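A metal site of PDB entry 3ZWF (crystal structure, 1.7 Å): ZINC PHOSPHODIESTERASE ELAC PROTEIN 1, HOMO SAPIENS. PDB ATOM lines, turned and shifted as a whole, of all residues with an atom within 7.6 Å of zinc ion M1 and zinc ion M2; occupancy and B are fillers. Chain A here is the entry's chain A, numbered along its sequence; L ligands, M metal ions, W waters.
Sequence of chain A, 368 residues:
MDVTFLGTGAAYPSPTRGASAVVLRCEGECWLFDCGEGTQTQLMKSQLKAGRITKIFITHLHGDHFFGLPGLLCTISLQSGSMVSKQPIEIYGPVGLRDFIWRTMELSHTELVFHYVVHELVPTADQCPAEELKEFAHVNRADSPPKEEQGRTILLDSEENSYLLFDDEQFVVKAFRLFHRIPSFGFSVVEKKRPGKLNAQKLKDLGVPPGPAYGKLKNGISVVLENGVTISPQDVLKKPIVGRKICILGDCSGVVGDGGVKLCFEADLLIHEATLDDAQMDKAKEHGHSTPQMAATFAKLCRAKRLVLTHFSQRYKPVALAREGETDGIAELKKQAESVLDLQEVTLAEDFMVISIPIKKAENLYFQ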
ATOM      1  N   GLY A   9      22.190  21.762 -32.766  1.00  0.00           N
ATOM      2  CA  GLY A   9      21.363  20.591 -32.903  1.00  0.00           C
ATOM      3  C   GLY A   9      21.045  19.884 -31.609  1.00  0.00           C
ATOM      4  O   GLY A   9      21.793  19.971 -30.599  1.00  0.00           O
ATOM      5  N   ALA A  10      19.976  19.100 -31.666  1.00  0.00           N
ATOM      6  CA  ALA A  10      19.510  18.241 -30.558  1.00  0.00           C
ATOM      7  C   ALA A  10      20.124  16.859 -30.577  1.00  0.00           C
ATOM      8  O   ALA A  10      20.299  16.289 -31.634  1.00  0.00           O
ATOM      9  CB  ALA A  10      18.023  18.075 -30.590  1.00  0.00           C
ATOM     10  N   ALA A  11      20.435  16.367 -29.381  1.00  0.00           N
ATOM     11  CA  ALA A  11      20.721  14.954 -29.085  1.00  0.00           C
ATOM     12  C   ALA A  11      22.065  14.374 -29.558  1.00  0.00           C
ATOM     13  O   ALA A  11      22.594  13.475 -28.889  1.00  0.00           O
ATOM     14  CB  ALA A  11      19.535  14.061 -29.518  1.00  0.00           C
ATOM     15  N   TYR A  12      22.583  14.823 -30.690  1.00  0.00           N
ATOM     16  CA  TYR A  12      23.854  14.416 -31.238  1.00  0.00           C
ATOM     17  C   TYR A  12      24.334  15.400 -32.267  1.00  0.00           C
ATOM     18  O   TYR A  12      23.528  16.148 -32.828  1.00  0.00           O
ATOM     19  CB  TYR A  12      23.782  13.014 -31.874  1.00  0.00           C
ATOM     20  CG  TYR A  12      22.740  12.852 -32.911  1.00  0.00           C
ATOM     21  CD1 TYR A  12      21.440  12.475 -32.586  1.00  0.00           C
ATOM     22  CD2 TYR A  12      23.041  13.092 -34.259  1.00  0.00           C
ATOM     23  CE1 TYR A  12      20.512  12.294 -33.562  1.00  0.00           C
ATOM     24  CE2 TYR A  12      22.116  12.936 -35.214  1.00  0.00           C
ATOM     25  CZ  TYR A  12      20.852  12.535 -34.878  1.00  0.00           C
ATOM     26  OH  TYR A  12      19.915  12.386 -35.884  1.00  0.00           O
ATOM     27  N   SER A  20      25.317  20.701 -28.756  1.00  0.00           N
ATOM     28  CA  SER A  20      25.175  21.961 -27.999  1.00  0.00           C
ATOM     29  C   SER A  20      26.497  22.595 -27.564  1.00  0.00           C
ATOM     30  O   SER A  20      27.321  21.986 -26.897  1.00  0.00           O
ATOM     31  CB  SER A  20      24.272  21.738 -26.794  1.00  0.00           C
ATOM     32  OG  SER A  20      22.955  21.588 -27.302  1.00  0.00           O
ATOM     33  N   ASP A  34      27.907  24.713 -22.453  1.00  0.00           N
ATOM     34  CA  ASP A  34      27.816  23.346 -22.998  1.00  0.00           C
ATOM     35  C   ASP A  34      28.950  23.008 -23.958  1.00  0.00           C
ATOM     36  O   ASP A  34      29.625  23.870 -24.528  1.00  0.00           O
ATOM     37  CB  ASP A  34      26.421  23.030 -23.564  1.00  0.00           C
ATOM     38  CG  ASP A  34      25.351  22.825 -22.435  1.00  0.00           C
ATOM     39  OD1 ASP A  34      25.749  22.598 -21.317  1.00  0.00           O
ATOM     40  OD2 ASP A  34      24.137  22.851 -22.718  1.00  0.00           O
ATOM     41  N   THR A  59      25.045  22.537 -18.656  1.00  0.00           N
ATOM     42  CA  THR A  59      23.616  22.626 -18.230  1.00  0.00           C
ATOM     43  C   THR A  59      23.093  21.314 -17.648  1.00  0.00           C
ATOM     44  O   THR A  59      22.310  21.316 -16.723  1.00  0.00           O
ATOM     45  CB  THR A  59      22.697  23.012 -19.350  1.00  0.00           C
ATOM     46  OG1 THR A  59      22.816  22.078 -20.439  1.00  0.00           O
ATOM     47  CG2 THR A  59      23.004  24.446 -19.865  1.00  0.00           C
ATOM     48  N   HIS A  60      23.582  20.173 -18.164  1.00  0.00           N
ATOM     49  CA  HIS A  60      23.131  18.865 -17.713  1.00  0.00           C
ATOM     50  C   HIS A  60      24.032  17.786 -18.278  1.00  0.00           C
ATOM     51  O   HIS A  60      24.653  18.011 -19.299  1.00  0.00           O
ATOM     52  CB  HIS A  60      21.672  18.596 -18.028  1.00  0.00           C
ATOM     53  CG  HIS A  60      21.322  18.446 -19.476  1.00  0.00           C
ATOM     54  ND1 HIS A  60      21.384  19.477 -20.411  1.00  0.00           N
ATOM     55  CD2 HIS A  60      20.684  17.429 -20.099  1.00  0.00           C
ATOM     56  CE1 HIS A  60      20.923  19.040 -21.562  1.00  0.00           C
ATOM     57  NE2 HIS A  60      20.488  17.800 -21.412  1.00  0.00           N
ATOM     58  N   LEU A  61      24.005  16.645 -17.609  1.00  0.00           N
ATOM     59  CA  LEU A  61      24.884  15.533 -17.994  1.00  0.00           C
ATOM     60  C   LEU A  61      24.253  14.579 -19.007  1.00  0.00           C
ATOM     61  O   LEU A  61      24.238  13.352 -18.780  1.00  0.00           O
ATOM     62  CB  LEU A  61      25.348  14.798 -16.715  1.00  0.00           C
ATOM     63  CG  LEU A  61      26.183  15.650 -15.755  1.00  0.00           C
ATOM     64  CD1 LEU A  61      26.644  14.873 -14.516  1.00  0.00           C
ATOM     65  CD2 LEU A  61      27.392  16.230 -16.515  1.00  0.00           C
ATOM     66  N   HIS A  62      23.795  15.129 -20.132  1.00  0.00           N
ATOM     67  CA  HIS A  62      23.503  14.355 -21.348  1.00  0.00           C
ATOM     68  C   HIS A  62      24.670  14.536 -22.262  1.00  0.00           C
ATOM     69  O   HIS A  62      25.250  15.599 -22.323  1.00  0.00           O
ATOM     70  CB  HIS A  62      22.211  14.782 -22.014  1.00  0.00           C
ATOM     71  CG  HIS A  62      21.010  14.129 -21.425  1.00  0.00           C
ATOM     72  ND1 HIS A  62      19.751  14.653 -21.583  1.00  0.00           N
ATOM     73  CD2 HIS A  62      20.858  12.977 -20.733  1.00  0.00           C
ATOM     74  CE1 HIS A  62      18.875  13.852 -21.012  1.00  0.00           C
ATOM     75  NE2 HIS A  62      19.536  12.829 -20.468  1.00  0.00           N
ATOM     76  N   GLY A  63      25.066  13.481 -22.982  1.00  0.00           N
ATOM     77  CA  GLY A  63      26.306  13.511 -23.709  1.00  0.00           C
ATOM     78  C   GLY A  63      26.479  14.595 -24.760  1.00  0.00           C
ATOM     79  O   GLY A  63      27.601  15.083 -24.980  1.00  0.00           O
ATOM     80  N   ASP A  64      25.377  15.015 -25.378  1.00  0.00           N
ATOM     81  CA  ASP A  64      25.369  16.074 -26.377  1.00  0.00           C
ATOM     82  C   ASP A  64      25.642  17.472 -25.788  1.00  0.00           C
ATOM     83  O   ASP A  64      25.726  18.444 -26.537  1.00  0.00           O
ATOM     84  CB  ASP A  64      24.043  16.139 -27.220  1.00  0.00           C
ATOM     85  CG  ASP A  64      22.805  16.149 -26.408  1.00  0.00           C
ATOM     86  OD1 ASP A  64      22.637  15.338 -25.447  1.00  0.00           O
ATOM     87  OD2 ASP A  64      21.953  17.001 -26.748  1.00  0.00           O
ATOM     88  N   HIS A  65      25.804  17.507 -24.460  1.00  0.00           N
ATOM     89  CA  HIS A  65      26.187  18.734 -23.766  1.00  0.00           C
ATOM     90  C   HIS A  65      27.535  18.674 -23.044  1.00  0.00           C
ATOM     91  O   HIS A  65      27.959  19.695 -22.472  1.00  0.00           O
ATOM     92  CB  HIS A  65      25.032  19.142 -22.805  1.00  0.00           C
ATOM     93  CG  HIS A  65      23.732  19.283 -23.525  1.00  0.00           C
ATOM     94  ND1 HIS A  65      23.174  20.512 -23.832  1.00  0.00           N
ATOM     95  CD2 HIS A  65      22.912  18.359 -24.048  1.00  0.00           C
ATOM     96  CE1 HIS A  65      22.068  20.313 -24.513  1.00  0.00           C
ATOM     97  NE2 HIS A  65      21.895  19.013 -24.665  1.00  0.00           N
ATOM     98  N   HIS A 180      13.850  18.353 -16.729  1.00  0.00           N
ATOM     99  CA  HIS A 180      14.232  17.612 -17.904  1.00  0.00           C
ATOM    100  C   HIS A 180      14.215  16.114 -17.554  1.00  0.00           C
ATOM    101  O   HIS A 180      13.843  15.740 -16.427  1.00  0.00           O
ATOM    102  CB  HIS A 180      15.586  18.145 -18.384  1.00  0.00           C
ATOM    103  CG  HIS A 180      16.089  17.566 -19.692  1.00  0.00           C
ATOM    104  ND1 HIS A 180      15.320  17.470 -20.836  1.00  0.00           N
ATOM    105  CD2 HIS A 180      17.312  17.087 -20.007  1.00  0.00           C
ATOM    106  CE1 HIS A 180      16.061  16.916 -21.792  1.00  0.00           C
ATOM    107  NE2 HIS A 180      17.271  16.688 -21.324  1.00  0.00           N
ATOM    108  N   ARG A 181      14.614  15.243 -18.477  1.00  0.00           N
ATOM    109  CA  ARG A 181      14.683  13.806 -18.207  1.00  0.00           C
ATOM    110  C   ARG A 181      15.685  13.486 -17.105  1.00  0.00           C
ATOM    111  O   ARG A 181      15.528  12.539 -16.329  1.00  0.00           O
ATOM    112  CB  ARG A 181      15.080  13.004 -19.492  1.00  0.00           C
ATOM    113  CG  ARG A 181      14.133  13.132 -20.624  1.00  0.00           C
ATOM    114  CD  ARG A 181      14.306  11.995 -21.667  1.00  0.00           C
ATOM    115  NE  ARG A 181      15.682  11.778 -22.157  1.00  0.00           N
ATOM    116  CZ  ARG A 181      16.387  12.653 -22.883  1.00  0.00           C
ATOM    117  NH1 ARG A 181      15.913  13.868 -23.195  1.00  0.00           N
ATOM    118  NH2 ARG A 181      17.608  12.316 -23.279  1.00  0.00           N
ATOM    119  N   ILE A 182      16.740  14.305 -17.040  1.00  0.00           N
ATOM    120  CA  ILE A 182      17.666  14.319 -15.889  1.00  0.00           C
ATOM    121  C   ILE A 182      17.707  15.777 -15.459  1.00  0.00           C
ATOM    122  O   ILE A 182      17.233  16.639 -16.211  1.00  0.00           O
ATOM    123  CB  ILE A 182      19.077  13.797 -16.217  1.00  0.00           C
ATOM    124  CG1 ILE A 182      19.797  14.618 -17.270  1.00  0.00           C
ATOM    125  CG2 ILE A 182      18.990  12.312 -16.616  1.00  0.00           C
ATOM    126  CD1 ILE A 182      21.250  14.285 -17.389  1.00  0.00           C
ATOM    127  N   SER A 184      18.495  19.541 -15.073  1.00  0.00           N
ATOM    128  CA  SER A 184      19.084  20.460 -15.988  1.00  0.00           C
ATOM    129  C   SER A 184      18.993  21.876 -15.419  1.00  0.00           C
ATOM    130  O   SER A 184      18.130  22.163 -14.578  1.00  0.00           O
ATOM    131  CB  SER A 184      18.374  20.331 -17.353  1.00  0.00           C
ATOM    132  OG  SER A 184      18.873  21.243 -18.338  1.00  0.00           O
ATOM    133  N   GLY A 250      19.444  25.233 -20.395  1.00  0.00           N
ATOM    134  CA  GLY A 250      19.611  23.840 -20.859  1.00  0.00           C
ATOM    135  C   GLY A 250      18.305  23.224 -21.340  1.00  0.00           C
ATOM    136  O   GLY A 250      17.205  23.821 -21.234  1.00  0.00           O
ATOM    137  N   ASP A 251      18.415  22.008 -21.871  1.00  0.00           N
ATOM    138  CA  ASP A 251      17.244  21.226 -22.289  1.00  0.00           C
ATOM    139  C   ASP A 251      16.246  21.212 -21.146  1.00  0.00           C
ATOM    140  O   ASP A 251      16.590  21.053 -19.980  1.00  0.00           O
ATOM    141  CB  ASP A 251      17.584  19.780 -22.556  1.00  0.00           C
ATOM    142  CG  ASP A 251      18.560  19.573 -23.733  1.00  0.00           C
ATOM    143  OD1 ASP A 251      19.023  20.537 -24.361  1.00  0.00           O
ATOM    144  OD2 ASP A 251      18.906  18.392 -23.989  1.00  0.00           O
ATOM    145  N   CYS A 252      14.985  21.371 -21.507  1.00  0.00           N
ATOM    146  CA  CYS A 252      13.901  21.433 -20.506  1.00  0.00           C
ATOM    147  C   CYS A 252      12.531  21.408 -21.173  1.00  0.00           C
ATOM    148  O   CYS A 252      12.378  21.774 -22.321  1.00  0.00           O
ATOM    149  CB  CYS A 252      14.014  22.700 -19.664  1.00  0.00           C
ATOM    150  SG  CYS A 252      13.728  24.248 -20.482  1.00  0.00           S
ATOM    151  N   GLU A 273      15.830  26.097 -25.771  1.00  0.00           N
ATOM    152  CA  GLU A 273      15.594  25.015 -26.754  1.00  0.00           C
ATOM    153  C   GLU A 273      14.191  25.022 -27.383  1.00  0.00           C
ATOM    154  O   GLU A 273      13.209  25.505 -26.841  1.00  0.00           O
ATOM    155  CB  GLU A 273      15.811  23.649 -26.123  1.00  0.00           C
ATOM    156  CG  GLU A 273      14.783  23.258 -25.074  1.00  0.00           C
ATOM    157  CD  GLU A 273      14.434  21.796 -25.231  1.00  0.00           C
ATOM    158  OE1 GLU A 273      13.764  21.448 -26.240  1.00  0.00           O
ATOM    159  OE2 GLU A 273      14.894  20.984 -24.408  1.00  0.00           O
ATOM    160  N   THR A 275      13.194  21.805 -29.386  1.00  0.00           N
ATOM    161  CA  THR A 275      13.606  20.547 -30.021  1.00  0.00           C
ATOM    162  C   THR A 275      12.659  20.101 -31.153  1.00  0.00           C
ATOM    163  O   THR A 275      13.105  19.708 -32.248  1.00  0.00           O
ATOM    164  CB  THR A 275      13.828  19.397 -29.007  1.00  0.00           C
ATOM    165  OG1 THR A 275      14.811  19.804 -28.044  1.00  0.00           O
ATOM    166  CG2 THR A 275      14.273  18.135 -29.738  1.00  0.00           C
ATOM    167  N   HIS A 287       9.876  13.729 -23.561  1.00  0.00           N
ATOM    168  CA  HIS A 287      11.340  13.681 -23.547  1.00  0.00           C
ATOM    169  C   HIS A 287      12.007  14.831 -22.814  1.00  0.00           C
ATOM    170  O   HIS A 287      13.221  15.016 -22.941  1.00  0.00           O
ATOM    171  CB  HIS A 287      11.885  13.585 -24.966  1.00  0.00           C
ATOM    172  CG  HIS A 287      11.601  12.271 -25.609  1.00  0.00           C
ATOM    173  ND1 HIS A 287      10.490  12.048 -26.390  1.00  0.00           N
ATOM    174  CD2 HIS A 287      12.263  11.092 -25.553  1.00  0.00           C
ATOM    175  CE1 HIS A 287      10.491  10.801 -26.809  1.00  0.00           C
ATOM    176  NE2 HIS A 287      11.550  10.188 -26.307  1.00  0.00           N
ATOM    177  N   GLY A 288      11.225  15.591 -22.046  1.00  0.00           N
ATOM    178  CA  GLY A 288      11.761  16.728 -21.278  1.00  0.00           C
ATOM    179  C   GLY A 288      12.221  17.897 -22.132  1.00  0.00           C
ATOM    180  O   GLY A 288      13.152  18.641 -21.783  1.00  0.00           O
ATOM    181  N   HIS A 289      11.525  18.067 -23.268  1.00  0.00           N
ATOM    182  CA  HIS A 289      11.849  19.094 -24.240  1.00  0.00           C
ATOM    183  C   HIS A 289      10.704  20.127 -24.366  1.00  0.00           C
ATOM    184  O   HIS A 289       9.621  19.930 -23.837  1.00  0.00           O
ATOM    185  CB  HIS A 289      12.210  18.476 -25.598  1.00  0.00           C
ATOM    186  CG  HIS A 289      13.543  17.790 -25.604  1.00  0.00           C
ATOM    187  ND1 HIS A 289      14.686  18.393 -25.132  1.00  0.00           N
ATOM    188  CD2 HIS A 289      13.925  16.566 -26.053  1.00  0.00           C
ATOM    189  CE1 HIS A 289      15.715  17.563 -25.257  1.00  0.00           C
ATOM    190  NE2 HIS A 289      15.270  16.429 -25.785  1.00  0.00           N
ATOM    191  N   HIS A 311      18.891  24.025 -30.338  1.00  0.00           N
ATOM    192  CA  HIS A 311      18.697  22.599 -30.015  1.00  0.00           C
ATOM    193  C   HIS A 311      17.561  21.995 -30.801  1.00  0.00           C
ATOM    194  O   HIS A 311      16.703  21.328 -30.263  1.00  0.00           O
ATOM    195  CB  HIS A 311      18.491  22.391 -28.498  1.00  0.00           C
ATOM    196  CG  HIS A 311      18.704  20.989 -28.007  1.00  0.00           C
ATOM    197  ND1 HIS A 311      17.692  20.060 -27.915  1.00  0.00           N
ATOM    198  CD2 HIS A 311      19.788  20.415 -27.442  1.00  0.00           C
ATOM    199  CE1 HIS A 311      18.159  18.939 -27.390  1.00  0.00           C
ATOM    200  NE2 HIS A 311      19.425  19.143 -27.058  1.00  0.00           N
HETATM  201  P1  LIG L   1      18.300  15.181 -25.664  1.00  0.00           P
HETATM  202  O1  LIG L   1      17.907  15.485 -24.188  1.00  0.00           O
HETATM  203  O2  LIG L   1      19.385  13.982 -25.534  1.00  0.00           O
HETATM  204  O3  LIG L   1      19.062  16.294 -26.260  1.00  0.00           O
HETATM  205  O4  LIG L   1      17.089  14.654 -26.331  1.00  0.00           O
HETATM  206 ZN    ZN M   1      20.299  17.802 -25.566  1.00  0.00          ZN
HETATM  207 ZN    ZN M   2      19.118  16.431 -22.652  1.00  0.00          ZN
HETATM  208  O   HOH W   1      20.618  16.271 -24.066  1.00  0.00           O
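O3 of the ligand is bound to zinc ion M1 (2.1 Å).
Water W1 is bound to zinc ion M1, 2.2 Å away.
The side-chain carboxylate (OD2) of Asp 64 binds zinc ion M1.
Zinc ion M1 is bound by OD2 of Asp 251 (2.2 Å).
Zinc ion M1 is bound by NE2 of His 311 (2.2 Å).
A ring nitrogen (NE2) of His 65 is bound to zinc ion M1, 2.2 Å away.
Of the 26 residues printed, 4 come within 4 Å of zinc ion M2.
Along chain A the residues within 4 Å of zinc ion M2 span positions 60 to 251.
Zinc ion M2 is bound by water W1 (2.1 Å), a ring nitrogen (ND1) of His 62 (2.2 Å), an oxygen (O1) of the ligand (2.2 Å), a ring nitrogen (NE2) of His 180 (2.3 Å), a ring nitrogen (NE2) of His 60 (2.3 Å) and the side-chain carboxylate of Asp 251 (2.4 Å).
A ring nitrogen (NE2) of His 62 lies close to the guanidinium group (NH2) of Arg 181, 3.4 Å away.
N of Ala 11 sits close to OD2 of Asp 64, at 3.1 Å.
O of Asp 64 lies within hydrogen-bond range of N of Ser 20.
The backbone carbonyl oxygen (O) of Asp 251 sits at hydrogen-bond distance from the side-chain hydroxyl (OG) of Ser 184, at 2.8 Å.
OG1 of Thr 275 sits at hydrogen-bond distance from ND1 of His 311, 2.9 Å away.
A ring nitrogen (ND1) of His 65 is in hydrogen-bond range of the side-chain carboxylate (OD2) of Asp 34.
The backbone carbonyl oxygen (O) of Gly 288 is in hydrogen-bond range of a ring nitrogen (ND1) of His 180 (2.6 Å).
ND1 of His 60 is in hydrogen-bond range of OG1 of Thr 59 (3.0 Å).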
